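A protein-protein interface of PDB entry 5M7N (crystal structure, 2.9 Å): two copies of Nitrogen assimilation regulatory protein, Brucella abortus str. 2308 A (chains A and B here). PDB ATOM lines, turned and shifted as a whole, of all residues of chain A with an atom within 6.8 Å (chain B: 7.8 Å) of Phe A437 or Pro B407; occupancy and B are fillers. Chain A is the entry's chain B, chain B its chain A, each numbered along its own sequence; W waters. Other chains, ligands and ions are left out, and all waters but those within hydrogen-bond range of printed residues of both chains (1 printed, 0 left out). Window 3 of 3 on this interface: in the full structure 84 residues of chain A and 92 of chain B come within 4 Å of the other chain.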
ATOM      1  N   TYR A 419      10.162  19.491  25.184  1.00  0.00           N
ATOM      2  CA  TYR A 419       9.584  18.848  24.005  1.00  0.00           C
ATOM      3  C   TYR A 419       8.768  17.606  24.413  1.00  0.00           C
ATOM      4  O   TYR A 419       7.630  17.470  23.978  1.00  0.00           O
ATOM      5  CB  TYR A 419      10.701  18.483  22.998  1.00  0.00           C
ATOM      6  CG  TYR A 419      10.292  17.479  21.938  1.00  0.00           C
ATOM      7  CD1 TYR A 419       9.714  17.897  20.741  1.00  0.00           C
ATOM      8  CD2 TYR A 419      10.482  16.115  22.130  1.00  0.00           C
ATOM      9  CE1 TYR A 419       9.301  16.973  19.777  1.00  0.00           C
ATOM     10  CE2 TYR A 419      10.086  15.184  21.172  1.00  0.00           C
ATOM     11  CZ  TYR A 419       9.510  15.619  19.990  1.00  0.00           C
ATOM     12  OH  TYR A 419       9.123  14.692  19.062  1.00  0.00           O
ATOM     13  N   GLN A 423       4.775  16.902  24.406  1.00  0.00           N
ATOM     14  CA  GLN A 423       4.249  15.761  23.642  1.00  0.00           C
ATOM     15  C   GLN A 423       3.332  14.879  24.500  1.00  0.00           C
ATOM     16  O   GLN A 423       2.255  14.484  24.039  1.00  0.00           O
ATOM     17  CB  GLN A 423       5.370  14.960  22.959  1.00  0.00           C
ATOM     18  CG  GLN A 423       6.028  15.721  21.801  1.00  0.00           C
ATOM     19  CD  GLN A 423       5.346  15.610  20.448  1.00  0.00           C
ATOM     20  OE1 GLN A 423       4.184  15.230  20.323  1.00  0.00           O
ATOM     21  NE2 GLN A 423       6.063  15.966  19.388  1.00  0.00           N
ATOM     22  N   ARG A 426       0.203  16.781  24.884  1.00  0.00           N
ATOM     23  CA  ARG A 426      -0.505  16.697  23.598  1.00  0.00           C
ATOM     24  C   ARG A 426      -1.310  15.390  23.496  1.00  0.00           C
ATOM     25  O   ARG A 426      -2.475  15.432  23.107  1.00  0.00           O
ATOM     26  CB  ARG A 426       0.470  16.859  22.411  1.00  0.00           C
ATOM     27  CG  ARG A 426      -0.082  16.461  21.047  1.00  0.00           C
ATOM     28  CD  ARG A 426       1.032  16.354  20.019  1.00  0.00           C
ATOM     29  NE  ARG A 426       0.606  15.686  18.785  1.00  0.00           N
ATOM     30  CZ  ARG A 426       1.433  15.301  17.820  1.00  0.00           C
ATOM     31  NH1 ARG A 426       2.738  15.498  17.939  1.00  0.00           N
ATOM     32  NH2 ARG A 426       0.963  14.711  16.729  1.00  0.00           N
ATOM     33  N   PHE A 427      -0.704  14.252  23.899  1.00  0.00           N
ATOM     34  CA  PHE A 427      -1.333  12.926  23.853  1.00  0.00           C
ATOM     35  C   PHE A 427      -2.051  12.604  25.172  1.00  0.00           C
ATOM     36  O   PHE A 427      -2.378  11.445  25.433  1.00  0.00           O
ATOM     37  CB  PHE A 427      -0.293  11.836  23.494  1.00  0.00           C
ATOM     38  CG  PHE A 427       0.266  11.849  22.081  1.00  0.00           C
ATOM     39  CD1 PHE A 427       1.155  12.840  21.672  1.00  0.00           C
ATOM     40  CD2 PHE A 427      -0.023  10.823  21.191  1.00  0.00           C
ATOM     41  CE1 PHE A 427       1.691  12.835  20.382  1.00  0.00           C
ATOM     42  CE2 PHE A 427       0.526  10.815  19.904  1.00  0.00           C
ATOM     43  CZ  PHE A 427       1.367  11.828  19.506  1.00  0.00           C
ATOM     44  N   SER A 432       2.835   5.537  26.063  1.00  0.00           N
ATOM     45  CA  SER A 432       2.983   4.596  24.948  1.00  0.00           C
ATOM     46  C   SER A 432       2.743   5.254  23.576  1.00  0.00           C
ATOM     47  O   SER A 432       3.457   4.934  22.621  1.00  0.00           O
ATOM     48  CB  SER A 432       2.045   3.409  25.125  1.00  0.00           C
ATOM     49  OG  SER A 432       2.304   2.744  26.352  1.00  0.00           O
ATOM     50  N   ARG A 433       1.730   6.149  23.478  1.00  0.00           N
ATOM     51  CA  ARG A 433       1.411   6.861  22.233  1.00  0.00           C
ATOM     52  C   ARG A 433       2.457   7.905  21.945  1.00  0.00           C
ATOM     53  O   ARG A 433       2.880   8.048  20.791  1.00  0.00           O
ATOM     54  CB  ARG A 433       0.014   7.475  22.272  1.00  0.00           C
ATOM     55  CG  ARG A 433      -1.041   6.472  21.846  1.00  0.00           C
ATOM     56  CD  ARG A 433      -2.394   7.087  21.556  1.00  0.00           C
ATOM     57  NE  ARG A 433      -3.354   6.039  21.196  1.00  0.00           N
ATOM     58  CZ  ARG A 433      -4.470   5.778  21.868  1.00  0.00           C
ATOM     59  NH1 ARG A 433      -4.810   6.510  22.922  1.00  0.00           N
ATOM     60  NH2 ARG A 433      -5.271   4.797  21.472  1.00  0.00           N
ATOM     61  N   THR A 434       2.901   8.601  23.015  1.00  0.00           N
ATOM     62  CA  THR A 434       3.961   9.602  22.992  1.00  0.00           C
ATOM     63  C   THR A 434       5.232   8.940  22.440  1.00  0.00           C
ATOM     64  O   THR A 434       5.618   9.259  21.309  1.00  0.00           O
ATOM     65  CB  THR A 434       4.134  10.210  24.380  1.00  0.00           C
ATOM     66  OG1 THR A 434       2.858  10.674  24.843  1.00  0.00           O
ATOM     67  CG2 THR A 434       5.151  11.340  24.388  1.00  0.00           C
ATOM     68  N   ALA A 435       5.784   7.929  23.175  1.00  0.00           N
ATOM     69  CA  ALA A 435       6.948   7.123  22.791  1.00  0.00           C
ATOM     70  C   ALA A 435       6.937   6.705  21.317  1.00  0.00           C
ATOM     71  O   ALA A 435       7.917   6.942  20.625  1.00  0.00           O
ATOM     72  CB  ALA A 435       7.055   5.896  23.677  1.00  0.00           C
ATOM     73  N   GLU A 436       5.825   6.148  20.820  1.00  0.00           N
ATOM     74  CA  GLU A 436       5.735   5.727  19.433  1.00  0.00           C
ATOM     75  C   GLU A 436       5.875   6.875  18.445  1.00  0.00           C
ATOM     76  O   GLU A 436       6.625   6.730  17.465  1.00  0.00           O
ATOM     77  CB  GLU A 436       4.463   4.921  19.157  1.00  0.00           C
ATOM     78  CG  GLU A 436       4.716   3.856  18.096  1.00  0.00           C
ATOM     79  CD  GLU A 436       3.519   3.076  17.600  1.00  0.00           C
ATOM     80  OE1 GLU A 436       2.875   2.381  18.418  1.00  0.00           O
ATOM     81  OE2 GLU A 436       3.279   3.095  16.372  1.00  0.00           O
ATOM     82  N   PHE A 437       5.169   8.019  18.708  1.00  0.00           N
ATOM     83  CA  PHE A 437       5.222   9.224  17.866  1.00  0.00           C
ATOM     84  C   PHE A 437       6.623   9.849  17.870  1.00  0.00           C
ATOM     85  O   PHE A 437       7.159  10.160  16.807  1.00  0.00           O
ATOM     86  CB  PHE A 437       4.176  10.274  18.285  1.00  0.00           C
ATOM     87  CG  PHE A 437       4.250  11.506  17.408  1.00  0.00           C
ATOM     88  CD1 PHE A 437       3.589  11.551  16.191  1.00  0.00           C
ATOM     89  CD2 PHE A 437       5.088  12.567  17.739  1.00  0.00           C
ATOM     90  CE1 PHE A 437       3.726  12.648  15.349  1.00  0.00           C
ATOM     91  CE2 PHE A 437       5.247  13.645  16.878  1.00  0.00           C
ATOM     92  CZ  PHE A 437       4.535  13.697  15.708  1.00  0.00           C
ATOM     93  N   VAL A 438       7.172  10.059  19.075  1.00  0.00           N
ATOM     94  CA  VAL A 438       8.497  10.577  19.402  1.00  0.00           C
ATOM     95  C   VAL A 438       9.654   9.730  18.772  1.00  0.00           C
ATOM     96  O   VAL A 438      10.705  10.278  18.416  1.00  0.00           O
ATOM     97  CB  VAL A 438       8.569  10.701  20.946  1.00  0.00           C
ATOM     98  CG1 VAL A 438       9.992  10.747  21.466  1.00  0.00           C
ATOM     99  CG2 VAL A 438       7.770  11.909  21.433  1.00  0.00           C
ATOM    100  N   GLY A 439       9.421   8.424  18.616  1.00  0.00           N
ATOM    101  CA  GLY A 439      10.378   7.489  18.030  1.00  0.00           C
ATOM    102  C   GLY A 439      11.178   6.721  19.063  1.00  0.00           C
ATOM    103  O   GLY A 439      12.318   6.310  18.812  1.00  0.00           O
ATOM    104  N   MET A 440      10.572   6.520  20.235  1.00  0.00           N
ATOM    105  CA  MET A 440      11.152   5.817  21.370  1.00  0.00           C
ATOM    106  C   MET A 440      10.329   4.586  21.787  1.00  0.00           C
ATOM    107  O   MET A 440       9.162   4.439  21.408  1.00  0.00           O
ATOM    108  CB  MET A 440      11.276   6.777  22.569  1.00  0.00           C
ATOM    109  CG  MET A 440      12.375   7.792  22.422  1.00  0.00           C
ATOM    110  SD  MET A 440      12.584   8.786  23.905  1.00  0.00           S
ATOM    111  CE  MET A 440      13.768   7.808  24.801  1.00  0.00           C
ATOM    112  N   GLN B 401       3.117  23.935  16.538  1.00  0.00           N
ATOM    113  CA  GLN B 401       2.675  22.944  15.543  1.00  0.00           C
ATOM    114  C   GLN B 401       3.796  22.318  14.708  1.00  0.00           C
ATOM    115  O   GLN B 401       3.750  21.133  14.396  1.00  0.00           O
ATOM    116  CB  GLN B 401       1.593  23.544  14.628  1.00  0.00           C
ATOM    117  N   HIS B 402       4.782  23.125  14.356  1.00  0.00           N
ATOM    118  CA  HIS B 402       5.962  22.785  13.563  1.00  0.00           C
ATOM    119  C   HIS B 402       6.902  21.793  14.295  1.00  0.00           C
ATOM    120  O   HIS B 402       7.336  20.806  13.690  1.00  0.00           O
ATOM    121  CB  HIS B 402       6.697  24.090  13.174  1.00  0.00           C
ATOM    122  CG  HIS B 402       6.895  25.045  14.324  1.00  0.00           C
ATOM    123  ND1 HIS B 402       5.818  25.624  14.985  1.00  0.00           N
ATOM    124  CD2 HIS B 402       8.041  25.485  14.895  1.00  0.00           C
ATOM    125  CE1 HIS B 402       6.343  26.382  15.933  1.00  0.00           C
ATOM    126  NE2 HIS B 402       7.675  26.338  15.916  1.00  0.00           N
ATOM    127  N   ILE B 403       7.202  22.062  15.592  1.00  0.00           N
ATOM    128  CA  ILE B 403       8.065  21.234  16.443  1.00  0.00           C
ATOM    129  C   ILE B 403       7.343  19.933  16.822  1.00  0.00           C
ATOM    130  O   ILE B 403       7.930  18.854  16.695  1.00  0.00           O
ATOM    131  CB  ILE B 403       8.586  22.017  17.687  1.00  0.00           C
ATOM    132  CG1 ILE B 403       9.539  23.172  17.299  1.00  0.00           C
ATOM    133  CG2 ILE B 403       9.228  21.088  18.723  1.00  0.00           C
ATOM    134  CD1 ILE B 403      11.080  22.777  17.060  1.00  0.00           C
ATOM    135  N   MET B 404       6.073  20.038  17.276  1.00  0.00           N
ATOM    136  CA  MET B 404       5.254  18.890  17.683  1.00  0.00           C
ATOM    137  C   MET B 404       5.065  17.865  16.575  1.00  0.00           C
ATOM    138  O   MET B 404       5.020  16.679  16.877  1.00  0.00           O
ATOM    139  CB  MET B 404       3.903  19.312  18.274  1.00  0.00           C
ATOM    140  CG  MET B 404       4.005  20.153  19.516  1.00  0.00           C
ATOM    141  SD  MET B 404       4.543  19.246  20.960  1.00  0.00           S
ATOM    142  CE  MET B 404       6.250  19.804  21.077  1.00  0.00           C
ATOM    143  N   ALA B 405       5.014  18.308  15.302  1.00  0.00           N
ATOM    144  CA  ALA B 405       4.866  17.426  14.134  1.00  0.00           C
ATOM    145  C   ALA B 405       6.124  16.571  13.838  1.00  0.00           C
ATOM    146  O   ALA B 405       6.053  15.660  12.999  1.00  0.00           O
ATOM    147  CB  ALA B 405       4.484  18.239  12.910  1.00  0.00           C
ATOM    148  N   LEU B 406       7.256  16.850  14.541  1.00  0.00           N
ATOM    149  CA  LEU B 406       8.527  16.137  14.381  1.00  0.00           C
ATOM    150  C   LEU B 406       8.852  15.159  15.521  1.00  0.00           C
ATOM    151  O   LEU B 406       8.636  15.513  16.677  1.00  0.00           O
ATOM    152  CB  LEU B 406       9.669  17.154  14.283  1.00  0.00           C
ATOM    153  CG  LEU B 406       9.751  18.004  13.040  1.00  0.00           C
ATOM    154  CD1 LEU B 406      10.533  19.257  13.325  1.00  0.00           C
ATOM    155  CD2 LEU B 406      10.417  17.246  11.937  1.00  0.00           C
ATOM    156  N   PRO B 407       9.455  13.966  15.237  1.00  0.00           N
ATOM    157  CA  PRO B 407       9.854  13.045  16.335  1.00  0.00           C
ATOM    158  C   PRO B 407      11.120  13.561  17.047  1.00  0.00           C
ATOM    159  O   PRO B 407      11.759  14.484  16.542  1.00  0.00           O
ATOM    160  CB  PRO B 407      10.111  11.711  15.611  1.00  0.00           C
ATOM    161  CG  PRO B 407       9.663  11.932  14.166  1.00  0.00           C
ATOM    162  CD  PRO B 407       9.812  13.394  13.926  1.00  0.00           C
ATOM    163  N   LEU B 408      11.473  13.001  18.222  1.00  0.00           N
ATOM    164  CA  LEU B 408      12.609  13.478  19.037  1.00  0.00           C
ATOM    165  C   LEU B 408      13.917  13.833  18.252  1.00  0.00           C
ATOM    166  O   LEU B 408      14.266  15.010  18.235  1.00  0.00           O
ATOM    167  CB  LEU B 408      12.951  12.548  20.220  1.00  0.00           C
ATOM    168  CG  LEU B 408      14.044  13.068  21.185  1.00  0.00           C
ATOM    169  CD1 LEU B 408      13.730  14.470  21.729  1.00  0.00           C
ATOM    170  CD2 LEU B 408      14.282  12.104  22.305  1.00  0.00           C
ATOM    171  N   ARG B 409      14.620  12.855  17.616  1.00  0.00           N
ATOM    172  CA  ARG B 409      15.882  13.104  16.871  1.00  0.00           C
ATOM    173  C   ARG B 409      15.784  14.273  15.872  1.00  0.00           C
ATOM    174  O   ARG B 409      16.666  15.115  15.827  1.00  0.00           O
ATOM    175  CB  ARG B 409      16.388  11.833  16.163  1.00  0.00           C
ATOM    176  CG  ARG B 409      17.796  12.022  15.579  1.00  0.00           C
ATOM    177  CD  ARG B 409      18.400  10.819  14.888  1.00  0.00           C
ATOM    178  NE  ARG B 409      17.599  10.374  13.745  1.00  0.00           N
ATOM    179  CZ  ARG B 409      17.679  10.875  12.515  1.00  0.00           C
ATOM    180  NH1 ARG B 409      18.527  11.853  12.243  1.00  0.00           N
ATOM    181  NH2 ARG B 409      16.899  10.407  11.552  1.00  0.00           N
ATOM    182  N   GLU B 410      14.695  14.338  15.107  1.00  0.00           N
ATOM    183  CA  GLU B 410      14.439  15.395  14.136  1.00  0.00           C
ATOM    184  C   GLU B 410      14.217  16.727  14.803  1.00  0.00           C
ATOM    185  O   GLU B 410      14.720  17.727  14.307  1.00  0.00           O
ATOM    186  CB  GLU B 410      13.238  15.027  13.259  1.00  0.00           C
ATOM    187  CG  GLU B 410      13.619  14.007  12.194  1.00  0.00           C
ATOM    188  CD  GLU B 410      13.467  12.530  12.498  1.00  0.00           C
ATOM    189  OE1 GLU B 410      13.285  12.146  13.678  1.00  0.00           O
ATOM    190  OE2 GLU B 410      13.494  11.751  11.520  1.00  0.00           O
ATOM    191  N   ALA B 411      13.483  16.746  15.928  1.00  0.00           N
ATOM    192  CA  ALA B 411      13.188  17.958  16.668  1.00  0.00           C
ATOM    193  C   ALA B 411      14.472  18.506  17.269  1.00  0.00           C
ATOM    194  O   ALA B 411      14.760  19.696  17.104  1.00  0.00           O
ATOM    195  CB  ALA B 411      12.154  17.676  17.731  1.00  0.00           C
ATOM    196  N   ARG B 412      15.295  17.604  17.852  1.00  0.00           N
ATOM    197  CA  ARG B 412      16.606  17.866  18.458  1.00  0.00           C
ATOM    198  C   ARG B 412      17.629  18.419  17.443  1.00  0.00           C
ATOM    199  O   ARG B 412      18.327  19.377  17.770  1.00  0.00           O
ATOM    200  CB  ARG B 412      17.118  16.577  19.094  1.00  0.00           C
ATOM    201  CG  ARG B 412      18.348  16.731  19.967  1.00  0.00           C
ATOM    202  CD  ARG B 412      18.599  15.468  20.764  1.00  0.00           C
ATOM    203  NE  ARG B 412      18.831  14.305  19.910  1.00  0.00           N
ATOM    204  CZ  ARG B 412      18.439  13.069  20.200  1.00  0.00           C
ATOM    205  NH1 ARG B 412      17.782  12.822  21.327  1.00  0.00           N
ATOM    206  NH2 ARG B 412      18.692  12.073  19.362  1.00  0.00           N
ATOM    207  N   GLU B 413      17.700  17.851  16.218  1.00  0.00           N
ATOM    208  CA  GLU B 413      18.626  18.328  15.171  1.00  0.00           C
ATOM    209  C   GLU B 413      18.257  19.713  14.658  1.00  0.00           C
ATOM    210  O   GLU B 413      19.151  20.509  14.392  1.00  0.00           O
ATOM    211  CB  GLU B 413      18.726  17.355  13.991  1.00  0.00           C
ATOM    212  CG  GLU B 413      19.437  16.058  14.329  1.00  0.00           C
ATOM    213  CD  GLU B 413      19.582  15.063  13.195  1.00  0.00           C
ATOM    214  OE1 GLU B 413      18.981  15.272  12.111  1.00  0.00           O
ATOM    215  OE2 GLU B 413      20.301  14.059  13.402  1.00  0.00           O
HETATM  216  O   HOH W   1      13.434   9.936  17.250  1.00  0.00           O
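No position is printed for both chains.
OH of Tyr A419 lies within hydrogen-bond range of NE2 of Gln A423, at 3.3 Å. The side-chain amide oxygen of Gln A423 lies within hydrogen-bond range of the guanidinium group of Arg A426 (2.8 Å).
Water W1 lies within hydrogen-bond range of O of Val A438 (3.0 Å) and N of Arg B409 (3.2 Å).
Tyr A419 touches Ile B403. CD1 of Tyr A419 touches CE of Met B404, 3.97 Å away. Pro B407 touches Tyr A419. CE1 of Tyr A419 touches CB of Ala B411, at 3.6 Å. Gln A423 touches Leu B406. O of Met B404 touches CE2 of Phe A437, 3.0 Å away. Phe A437 touches Ala B405 (CZ to O, 3.7 Å). Leu B406 touches Phe A437. Pro B407 touches Phe A437. O of Val A438 touches CB of Pro B407, at 3.2 Å.
Phe A437 touches four residues of chain B. Of chain A, only Tyr A419 (3.1 Å), Phe A437 (3.5 Å) and Val A438 (3.2 Å) come within 4 Å of Pro B407. Printed residues of chain A within 4 Å of Ala B411: Tyr A419 (3.6 Å). Of the printed residues of chain A, Leu B408 touches Tyr A419 and Val A438. Printed residues of chain A within 4 Å of Ala B405: Phe A437 (3.7 Å). Printed residues of chain B within 4 Å of Tyr A419: Ile B403, Met B404, Leu B406, Pro B407, Leu B408 and Ala B411. Arg A433 touches none of the printed residues of chain B.
The side-chain hydroxyl (OH) of Tyr A419 is in hydrogen-bond range of the backbone carbonyl oxygen (O) of Leu B406, 2.6 Å away. The side-chain amide nitrogen of Gln A423 is in hydrogen-bond range of the backbone carbonyl oxygen of Met B404, at 2.8 Å. N of Leu B408 is in hydrogen-bond range of O of Val A438 (2.8 Å). N of Leu B408 is in hydrogen-bond range of OH of Tyr A419, 3.0 Å away. O of Met B404 sits at hydrogen-bond distance from NH1 of Arg A426.
Of the 13 printed residues of chain B, 7 touch a printed residue of chain A. Hydrophobic or aromatic side chains of chain B that line the printed part of chain A: Ile B403, Met B404, Pro B407, Leu B408 and Ala B411. Of the 13 printed residues of chain A, 5 touch a printed residue of chain B. Among the printed residues, 15 pairs touch across the chains. Among the printed residues, no Asp or Glu carboxylate lies within 4 Å of a Lys or Arg side-chain nitrogen of the other chain.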
